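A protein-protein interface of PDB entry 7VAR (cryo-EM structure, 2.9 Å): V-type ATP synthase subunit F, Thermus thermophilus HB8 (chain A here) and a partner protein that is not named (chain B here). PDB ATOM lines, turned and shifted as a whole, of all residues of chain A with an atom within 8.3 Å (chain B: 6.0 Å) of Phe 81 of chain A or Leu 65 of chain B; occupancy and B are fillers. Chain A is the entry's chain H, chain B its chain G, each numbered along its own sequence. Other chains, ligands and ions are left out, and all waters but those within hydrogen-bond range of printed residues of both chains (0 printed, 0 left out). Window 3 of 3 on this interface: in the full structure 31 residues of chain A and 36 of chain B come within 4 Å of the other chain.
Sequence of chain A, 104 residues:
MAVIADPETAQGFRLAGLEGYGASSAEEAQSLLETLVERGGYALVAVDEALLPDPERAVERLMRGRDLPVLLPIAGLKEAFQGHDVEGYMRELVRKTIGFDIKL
Among the printed residues, merely in contact across the chains: Glu 8 of chain A with Leu 64 of chain B (3.9 Å), Thr 9 of chain A with Tyr 61 of chain B (3.3 Å), Ala 75 of chain A with Tyr 61 of chain B (3.6 Å), Gly 76 of chain A with Tyr 61 of chain B (3.2 Å), Leu 77 of chain A with Tyr 61 of chain B (3.5 Å), Leu 77 of chain A with Leu 64 of chain B (3.7 Å), Ala 80 of chain A with Lys 58 of chain B (3.3 Å), Ala 80 of chain A with Tyr 61 of chain B (3.6 Å), Phe 81 of chain A with Tyr 61 of chain B (3.5 Å), Phe 81 of chain A with Ala 62 of chain B (3.6 Å) and Phe 81 of chain A with Leu 65 of chain B (3.5 Å).
NE2 of Gln 68 of chain B lies within hydrogen-bond range of O of Leu 65 of chain B, 3.1 Å away. The backbone NH (N) of Leu 77 of chain A lies close to the side-chain hydroxyl (OG1) of Thr 9 of chain A, at 3.3 Å.
Phe 81 of chain A touches three residues of chain B. Leu 65 of chain B touches just one residue of chain A: Phe 81. Printed residues of chain B within 4 Å of Leu 77 of chain A: Tyr 61 (3.5 Å) and Leu 64 (3.7 Å). Of the printed residues of chain B, Glu 8 of chain A touches Leu 64. Of the printed residues of chain B, Thr 9 of chain A touches Tyr 61. Printed residues of chain B within 4 Å of Ala 80 of chain A: Lys 58 and Tyr 61. The nearest printed residue of chain B that does not touch Ala 80 of chain A is Ala 62 of chain B (7.9 Å).
Printed residues of chain B that touch a printed residue of chain A: Lys 58, Tyr 61, Ala 62, Leu 64 and Leu 65. Of the 12 printed residues of chain A, 7 touch a printed residue of chain B. Printed residues of chain A that touch a printed residue of chain B: Glu 8, Thr 9, Ala 75, Gly 76, Leu 77, Ala 80 and Phe 81. Hydrophobic or aromatic side chains of chain A that line the printed part of chain B: Leu 77, Ala 80 and Phe 81. Among the printed residues, 11 pairs touch across the chains. Among the printed residues, no Asp or Glu carboxylate lies within 4 Å of a Lys or Arg side-chain nitrogen of the other chain.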
ATOM      1  N   GLU A   8     -11.779  -9.950 -17.026  1.00  0.00           N
ATOM      2  CA  GLU A   8     -11.402 -11.214 -17.652  1.00  0.00           C
ATOM      3  C   GLU A   8     -10.567 -10.972 -18.905  1.00  0.00           C
ATOM      4  O   GLU A   8      -9.565 -11.655 -19.141  1.00  0.00           O
ATOM      5  CB  GLU A   8     -12.651 -12.032 -17.985  1.00  0.00           C
ATOM      6  CG  GLU A   8     -13.514 -12.379 -16.784  1.00  0.00           C
ATOM      7  CD  GLU A   8     -14.741 -11.496 -16.678  1.00  0.00           C
ATOM      8  OE1 GLU A   8     -14.597 -10.260 -16.779  1.00  0.00           O
ATOM      9  OE2 GLU A   8     -15.852 -12.041 -16.498  1.00  0.00           O
ATOM     10  N   THR A   9     -10.974  -9.999 -19.724  1.00  0.00           N
ATOM     11  CA  THR A   9     -10.182  -9.629 -20.894  1.00  0.00           C
ATOM     12  C   THR A   9      -8.847  -9.023 -20.475  1.00  0.00           C
ATOM     13  O   THR A   9      -7.806  -9.300 -21.084  1.00  0.00           O
ATOM     14  CB  THR A   9     -10.967  -8.653 -21.770  1.00  0.00           C
ATOM     15  OG1 THR A   9     -12.195  -9.262 -22.183  1.00  0.00           O
ATOM     16  CG2 THR A   9     -10.170  -8.286 -23.002  1.00  0.00           C
ATOM     17  N   ALA A  75     -14.653  -5.087 -29.361  1.00  0.00           N
ATOM     18  CA  ALA A  75     -15.610  -5.798 -28.523  1.00  0.00           C
ATOM     19  C   ALA A  75     -14.919  -6.426 -27.317  1.00  0.00           C
ATOM     20  O   ALA A  75     -13.735  -6.771 -27.374  1.00  0.00           O
ATOM     21  CB  ALA A  75     -16.327  -6.872 -29.340  1.00  0.00           C
ATOM     22  N   GLY A  76     -15.663  -6.568 -26.224  1.00  0.00           N
ATOM     23  CA  GLY A  76     -15.145  -7.225 -25.039  1.00  0.00           C
ATOM     24  C   GLY A  76     -15.245  -8.736 -25.137  1.00  0.00           C
ATOM     25  O   GLY A  76     -15.543  -9.314 -26.182  1.00  0.00           O
ATOM     26  N   LEU A  77     -14.979  -9.393 -24.004  1.00  0.00           N
ATOM     27  CA  LEU A  77     -14.988 -10.852 -23.965  1.00  0.00           C
ATOM     28  C   LEU A  77     -16.370 -11.409 -24.288  1.00  0.00           C
ATOM     29  O   LEU A  77     -16.560 -12.092 -25.300  1.00  0.00           O
ATOM     30  CB  LEU A  77     -14.508 -11.339 -22.593  1.00  0.00           C
ATOM     31  CG  LEU A  77     -14.275 -12.839 -22.383  1.00  0.00           C
ATOM     32  CD1 LEU A  77     -13.165 -13.048 -21.374  1.00  0.00           C
ATOM     33  CD2 LEU A  77     -15.538 -13.546 -21.911  1.00  0.00           C
ATOM     34  N   LYS A  78     -17.351 -11.121 -23.432  1.00  0.00           N
ATOM     35  CA  LYS A  78     -18.702 -11.618 -23.672  1.00  0.00           C
ATOM     36  C   LYS A  78     -19.347 -10.923 -24.860  1.00  0.00           C
ATOM     37  O   LYS A  78     -20.225 -11.499 -25.514  1.00  0.00           O
ATOM     38  CB  LYS A  78     -19.559 -11.442 -22.419  1.00  0.00           C
ATOM     39  CG  LYS A  78     -20.602 -12.529 -22.226  1.00  0.00           C
ATOM     40  CD  LYS A  78     -19.968 -13.830 -21.759  1.00  0.00           C
ATOM     41  CE  LYS A  78     -21.022 -14.867 -21.409  1.00  0.00           C
ATOM     42  NZ  LYS A  78     -20.411 -16.150 -20.971  1.00  0.00           N
ATOM     43  N   GLU A  79     -18.932  -9.688 -25.150  1.00  0.00           N
ATOM     44  CA  GLU A  79     -19.453  -8.980 -26.313  1.00  0.00           C
ATOM     45  C   GLU A  79     -19.032  -9.668 -27.606  1.00  0.00           C
ATOM     46  O   GLU A  79     -19.818  -9.766 -28.555  1.00  0.00           O
ATOM     47  CB  GLU A  79     -18.983  -7.526 -26.290  1.00  0.00           C
ATOM     48  CG  GLU A  79     -19.465  -6.697 -27.467  1.00  0.00           C
ATOM     49  CD  GLU A  79     -20.977  -6.604 -27.542  1.00  0.00           C
ATOM     50  OE1 GLU A  79     -21.637  -6.664 -26.484  1.00  0.00           O
ATOM     51  OE2 GLU A  79     -21.506  -6.465 -28.665  1.00  0.00           O
ATOM     52  N   ALA A  80     -17.787 -10.147 -27.664  1.00  0.00           N
ATOM     53  CA  ALA A  80     -17.315 -10.844 -28.856  1.00  0.00           C
ATOM     54  C   ALA A  80     -17.947 -12.221 -29.011  1.00  0.00           C
ATOM     55  O   ALA A  80     -17.893 -12.791 -30.106  1.00  0.00           O
ATOM     56  CB  ALA A  80     -15.793 -10.976 -28.831  1.00  0.00           C
ATOM     57  N   PHE A  81     -18.537 -12.766 -27.951  1.00  0.00           N
ATOM     58  CA  PHE A  81     -19.207 -14.059 -28.053  1.00  0.00           C
ATOM     59  C   PHE A  81     -20.567 -13.964 -28.707  1.00  0.00           C
ATOM     60  O   PHE A  81     -21.182 -14.999 -28.997  1.00  0.00           O
ATOM     61  CB  PHE A  81     -19.333 -14.697 -26.670  1.00  0.00           C
ATOM     62  CG  PHE A  81     -18.109 -15.450 -26.241  1.00  0.00           C
ATOM     63  CD1 PHE A  81     -17.653 -16.528 -26.981  1.00  0.00           C
ATOM     64  CD2 PHE A  81     -17.414 -15.082 -25.103  1.00  0.00           C
ATOM     65  CE1 PHE A  81     -16.526 -17.225 -26.591  1.00  0.00           C
ATOM     66  CE2 PHE A  81     -16.288 -15.776 -24.709  1.00  0.00           C
ATOM     67  CZ  PHE A  81     -15.843 -16.849 -25.455  1.00  0.00           C
ATOM     68  N   GLN A  82     -21.049 -12.747 -28.944  1.00  0.00           N
ATOM     69  CA  GLN A  82     -22.274 -12.515 -29.689  1.00  0.00           C
ATOM     70  C   GLN A  82     -21.938 -11.718 -30.940  1.00  0.00           C
ATOM     71  O   GLN A  82     -20.941 -10.991 -30.980  1.00  0.00           O
ATOM     72  CB  GLN A  82     -23.326 -11.780 -28.841  1.00  0.00           C
ATOM     73  CG  GLN A  82     -22.954 -10.356 -28.459  1.00  0.00           C
ATOM     74  CD  GLN A  82     -23.610  -9.322 -29.354  1.00  0.00           C
ATOM     75  OE1 GLN A  82     -24.707  -9.537 -29.867  1.00  0.00           O
ATOM     76  NE2 GLN A  82     -22.939  -8.192 -29.544  1.00  0.00           N
ATOM     77  N   GLY A  83     -22.770 -11.876 -31.968  1.00  0.00           N
ATOM     78  CA  GLY A  83     -22.524 -11.252 -33.255  1.00  0.00           C
ATOM     79  C   GLY A  83     -22.349  -9.748 -33.192  1.00  0.00           C
ATOM     80  O   GLY A  83     -23.143  -9.047 -32.558  1.00  0.00           O
ATOM     81  N   HIS A  84     -21.306  -9.244 -33.845  1.00  0.00           N
ATOM     82  CA  HIS A  84     -20.996  -7.822 -33.868  1.00  0.00           C
ATOM     83  C   HIS A  84     -21.175  -7.290 -35.283  1.00  0.00           C
ATOM     84  O   HIS A  84     -20.582  -7.819 -36.229  1.00  0.00           O
ATOM     85  CB  HIS A  84     -19.568  -7.566 -33.381  1.00  0.00           C
ATOM     86  CG  HIS A  84     -19.296  -6.135 -33.034  1.00  0.00           C
ATOM     87  ND1 HIS A  84     -19.172  -5.150 -33.990  1.00  0.00           N
ATOM     88  CD2 HIS A  84     -19.123  -5.525 -31.840  1.00  0.00           C
ATOM     89  CE1 HIS A  84     -18.935  -3.992 -33.398  1.00  0.00           C
ATOM     90  NE2 HIS A  84     -18.899  -4.193 -32.092  1.00  0.00           N
ATOM     91  N   LYS B  58     -12.849 -13.955 -31.063  1.00  0.00           N
ATOM     92  CA  LYS B  58     -13.684 -15.094 -30.698  1.00  0.00           C
ATOM     93  C   LYS B  58     -12.832 -16.287 -30.287  1.00  0.00           C
ATOM     94  O   LYS B  58     -13.069 -16.905 -29.240  1.00  0.00           O
ATOM     95  CB  LYS B  58     -14.605 -15.471 -31.857  1.00  0.00           C
ATOM     96  CG  LYS B  58     -15.852 -14.615 -31.968  1.00  0.00           C
ATOM     97  CD  LYS B  58     -16.491 -14.762 -33.337  1.00  0.00           C
ATOM     98  CE  LYS B  58     -16.829 -16.214 -33.634  1.00  0.00           C
ATOM     99  NZ  LYS B  58     -17.989 -16.691 -32.831  1.00  0.00           N
ATOM    100  N   ALA B  60      -9.677 -16.330 -29.265  1.00  0.00           N
ATOM    101  CA  ALA B  60      -8.911 -16.057 -28.054  1.00  0.00           C
ATOM    102  C   ALA B  60      -9.781 -16.153 -26.809  1.00  0.00           C
ATOM    103  O   ALA B  60      -9.365 -16.734 -25.800  1.00  0.00           O
ATOM    104  CB  ALA B  60      -8.257 -14.679 -28.147  1.00  0.00           C
ATOM    105  N   TYR B  61     -10.992 -15.594 -26.857  1.00  0.00           N
ATOM    106  CA  TYR B  61     -11.873 -15.662 -25.697  1.00  0.00           C
ATOM    107  C   TYR B  61     -12.330 -17.094 -25.436  1.00  0.00           C
ATOM    108  O   TYR B  61     -12.440 -17.517 -24.277  1.00  0.00           O
ATOM    109  CB  TYR B  61     -13.068 -14.730 -25.889  1.00  0.00           C
ATOM    110  CG  TYR B  61     -12.695 -13.265 -25.856  1.00  0.00           C
ATOM    111  CD1 TYR B  61     -11.816 -12.775 -24.898  1.00  0.00           C
ATOM    112  CD2 TYR B  61     -13.225 -12.371 -26.776  1.00  0.00           C
ATOM    113  CE1 TYR B  61     -11.471 -11.437 -24.863  1.00  0.00           C
ATOM    114  CE2 TYR B  61     -12.883 -11.032 -26.751  1.00  0.00           C
ATOM    115  CZ  TYR B  61     -12.008 -10.571 -25.791  1.00  0.00           C
ATOM    116  OH  TYR B  61     -11.671  -9.237 -25.762  1.00  0.00           O
ATOM    117  N   ALA B  62     -12.592 -17.858 -26.501  1.00  0.00           N
ATOM    118  CA  ALA B  62     -12.959 -19.260 -26.327  1.00  0.00           C
ATOM    119  C   ALA B  62     -11.827 -20.043 -25.675  1.00  0.00           C
ATOM    120  O   ALA B  62     -12.063 -20.890 -24.804  1.00  0.00           O
ATOM    121  CB  ALA B  62     -13.339 -19.875 -27.674  1.00  0.00           C
ATOM    122  N   ALA B  63     -10.586 -19.778 -26.089  1.00  0.00           N
ATOM    123  CA  ALA B  63      -9.446 -20.431 -25.454  1.00  0.00           C
ATOM    124  C   ALA B  63      -9.304 -20.010 -23.997  1.00  0.00           C
ATOM    125  O   ALA B  63      -8.976 -20.832 -23.133  1.00  0.00           O
ATOM    126  CB  ALA B  63      -8.165 -20.125 -26.229  1.00  0.00           C
ATOM    127  N   LEU B  64      -9.539 -18.727 -23.704  1.00  0.00           N
ATOM    128  CA  LEU B  64      -9.365 -18.236 -22.340  1.00  0.00           C
ATOM    129  C   LEU B  64     -10.405 -18.821 -21.391  1.00  0.00           C
ATOM    130  O   LEU B  64     -10.096 -19.102 -20.227  1.00  0.00           O
ATOM    131  CB  LEU B  64      -9.423 -16.709 -22.315  1.00  0.00           C
ATOM    132  CG  LEU B  64      -9.341 -16.059 -20.929  1.00  0.00           C
ATOM    133  CD1 LEU B  64      -8.394 -14.880 -20.949  1.00  0.00           C
ATOM    134  CD2 LEU B  64     -10.717 -15.622 -20.444  1.00  0.00           C
ATOM    135  N   LEU B  65     -11.644 -18.999 -21.862  1.00  0.00           N
ATOM    136  CA  LEU B  65     -12.715 -19.444 -20.971  1.00  0.00           C
ATOM    137  C   LEU B  65     -12.381 -20.776 -20.307  1.00  0.00           C
ATOM    138  O   LEU B  65     -12.744 -21.007 -19.148  1.00  0.00           O
ATOM    139  CB  LEU B  65     -14.033 -19.547 -21.737  1.00  0.00           C
ATOM    140  CG  LEU B  65     -14.840 -18.256 -21.877  1.00  0.00           C
ATOM    141  CD1 LEU B  65     -16.239 -18.559 -22.387  1.00  0.00           C
ATOM    142  CD2 LEU B  65     -14.899 -17.510 -20.552  1.00  0.00           C
ATOM    143  N   LEU B  66     -11.692 -21.666 -21.023  1.00  0.00           N
ATOM    144  CA  LEU B  66     -11.315 -22.947 -20.436  1.00  0.00           C
ATOM    145  C   LEU B  66     -10.254 -22.773 -19.356  1.00  0.00           C
ATOM    146  O   LEU B  66     -10.248 -23.507 -18.359  1.00  0.00           O
ATOM    147  CB  LEU B  66     -10.824 -23.903 -21.522  1.00  0.00           C
ATOM    148  CG  LEU B  66     -11.882 -24.780 -22.195  1.00  0.00           C
ATOM    149  CD1 LEU B  66     -12.802 -23.953 -23.082  1.00  0.00           C
ATOM    150  CD2 LEU B  66     -11.224 -25.895 -22.993  1.00  0.00           C
ATOM    151  N   ALA B  67      -9.344 -21.812 -19.538  1.00  0.00           N
ATOM    152  CA  ALA B  67      -8.252 -21.629 -18.586  1.00  0.00           C
ATOM    153  C   ALA B  67      -8.775 -21.234 -17.210  1.00  0.00           C
ATOM    154  O   ALA B  67      -8.296 -21.731 -16.186  1.00  0.00           O
ATOM    155  CB  ALA B  67      -7.271 -20.581 -19.111  1.00  0.00           C
ATOM    156  N   GLN B  68      -9.761 -20.335 -17.164  1.00  0.00           N
ATOM    157  CA  GLN B  68     -10.288 -19.888 -15.881  1.00  0.00           C
ATOM    158  C   GLN B  68     -11.198 -20.923 -15.232  1.00  0.00           C
ATOM    159  O   GLN B  68     -11.532 -20.780 -14.050  1.00  0.00           O
ATOM    160  CB  GLN B  68     -11.028 -18.557 -16.050  1.00  0.00           C
ATOM    161  CG  GLN B  68     -12.250 -18.606 -16.958  1.00  0.00           C
ATOM    162  CD  GLN B  68     -13.523 -18.965 -16.217  1.00  0.00           C
ATOM    163  OE1 GLN B  68     -13.967 -18.234 -15.331  1.00  0.00           O
ATOM    164  NE2 GLN B  68     -14.121 -20.092 -16.580  1.00  0.00           N
ATOM    165  N   ALA B  69     -11.604 -21.957 -15.968  1.00  0.00           N
ATOM    166  CA  ALA B  69     -12.468 -22.996 -15.419  1.00  0.00           C
ATOM    167  C   ALA B  69     -11.683 -24.233 -14.996  1.00  0.00           C
ATOM    168  O   ALA B  69     -11.736 -24.634 -13.829  1.00  0.00           O
ATOM    169  CB  ALA B  69     -13.545 -23.378 -16.440  1.00  0.00           C
ATOM    170  N   PHE B  70     -10.952 -24.848 -15.926  1.00  0.00           N
ATOM    171  CA  PHE B  70     -10.191 -26.051 -15.613  1.00  0.00           C
ATOM    172  C   PHE B  70      -8.971 -25.765 -14.750  1.00  0.00           C
ATOM    173  O   PHE B  70      -8.716 -26.501 -13.790  1.00  0.00           O
ATOM    174  CB  PHE B  70      -9.757 -26.758 -16.902  1.00  0.00           C
ATOM    175  CG  PHE B  70     -10.904 -27.189 -17.772  1.00  0.00           C
ATOM    176  CD1 PHE B  70     -12.148 -27.454 -17.224  1.00  0.00           C
ATOM    177  CD2 PHE B  70     -10.736 -27.335 -19.140  1.00  0.00           C
ATOM    178  CE1 PHE B  70     -13.204 -27.852 -18.022  1.00  0.00           C
ATOM    179  CE2 PHE B  70     -11.788 -27.733 -19.943  1.00  0.00           C
ATOM    180  CZ  PHE B  70     -13.023 -27.992 -19.383  1.00  0.00           C
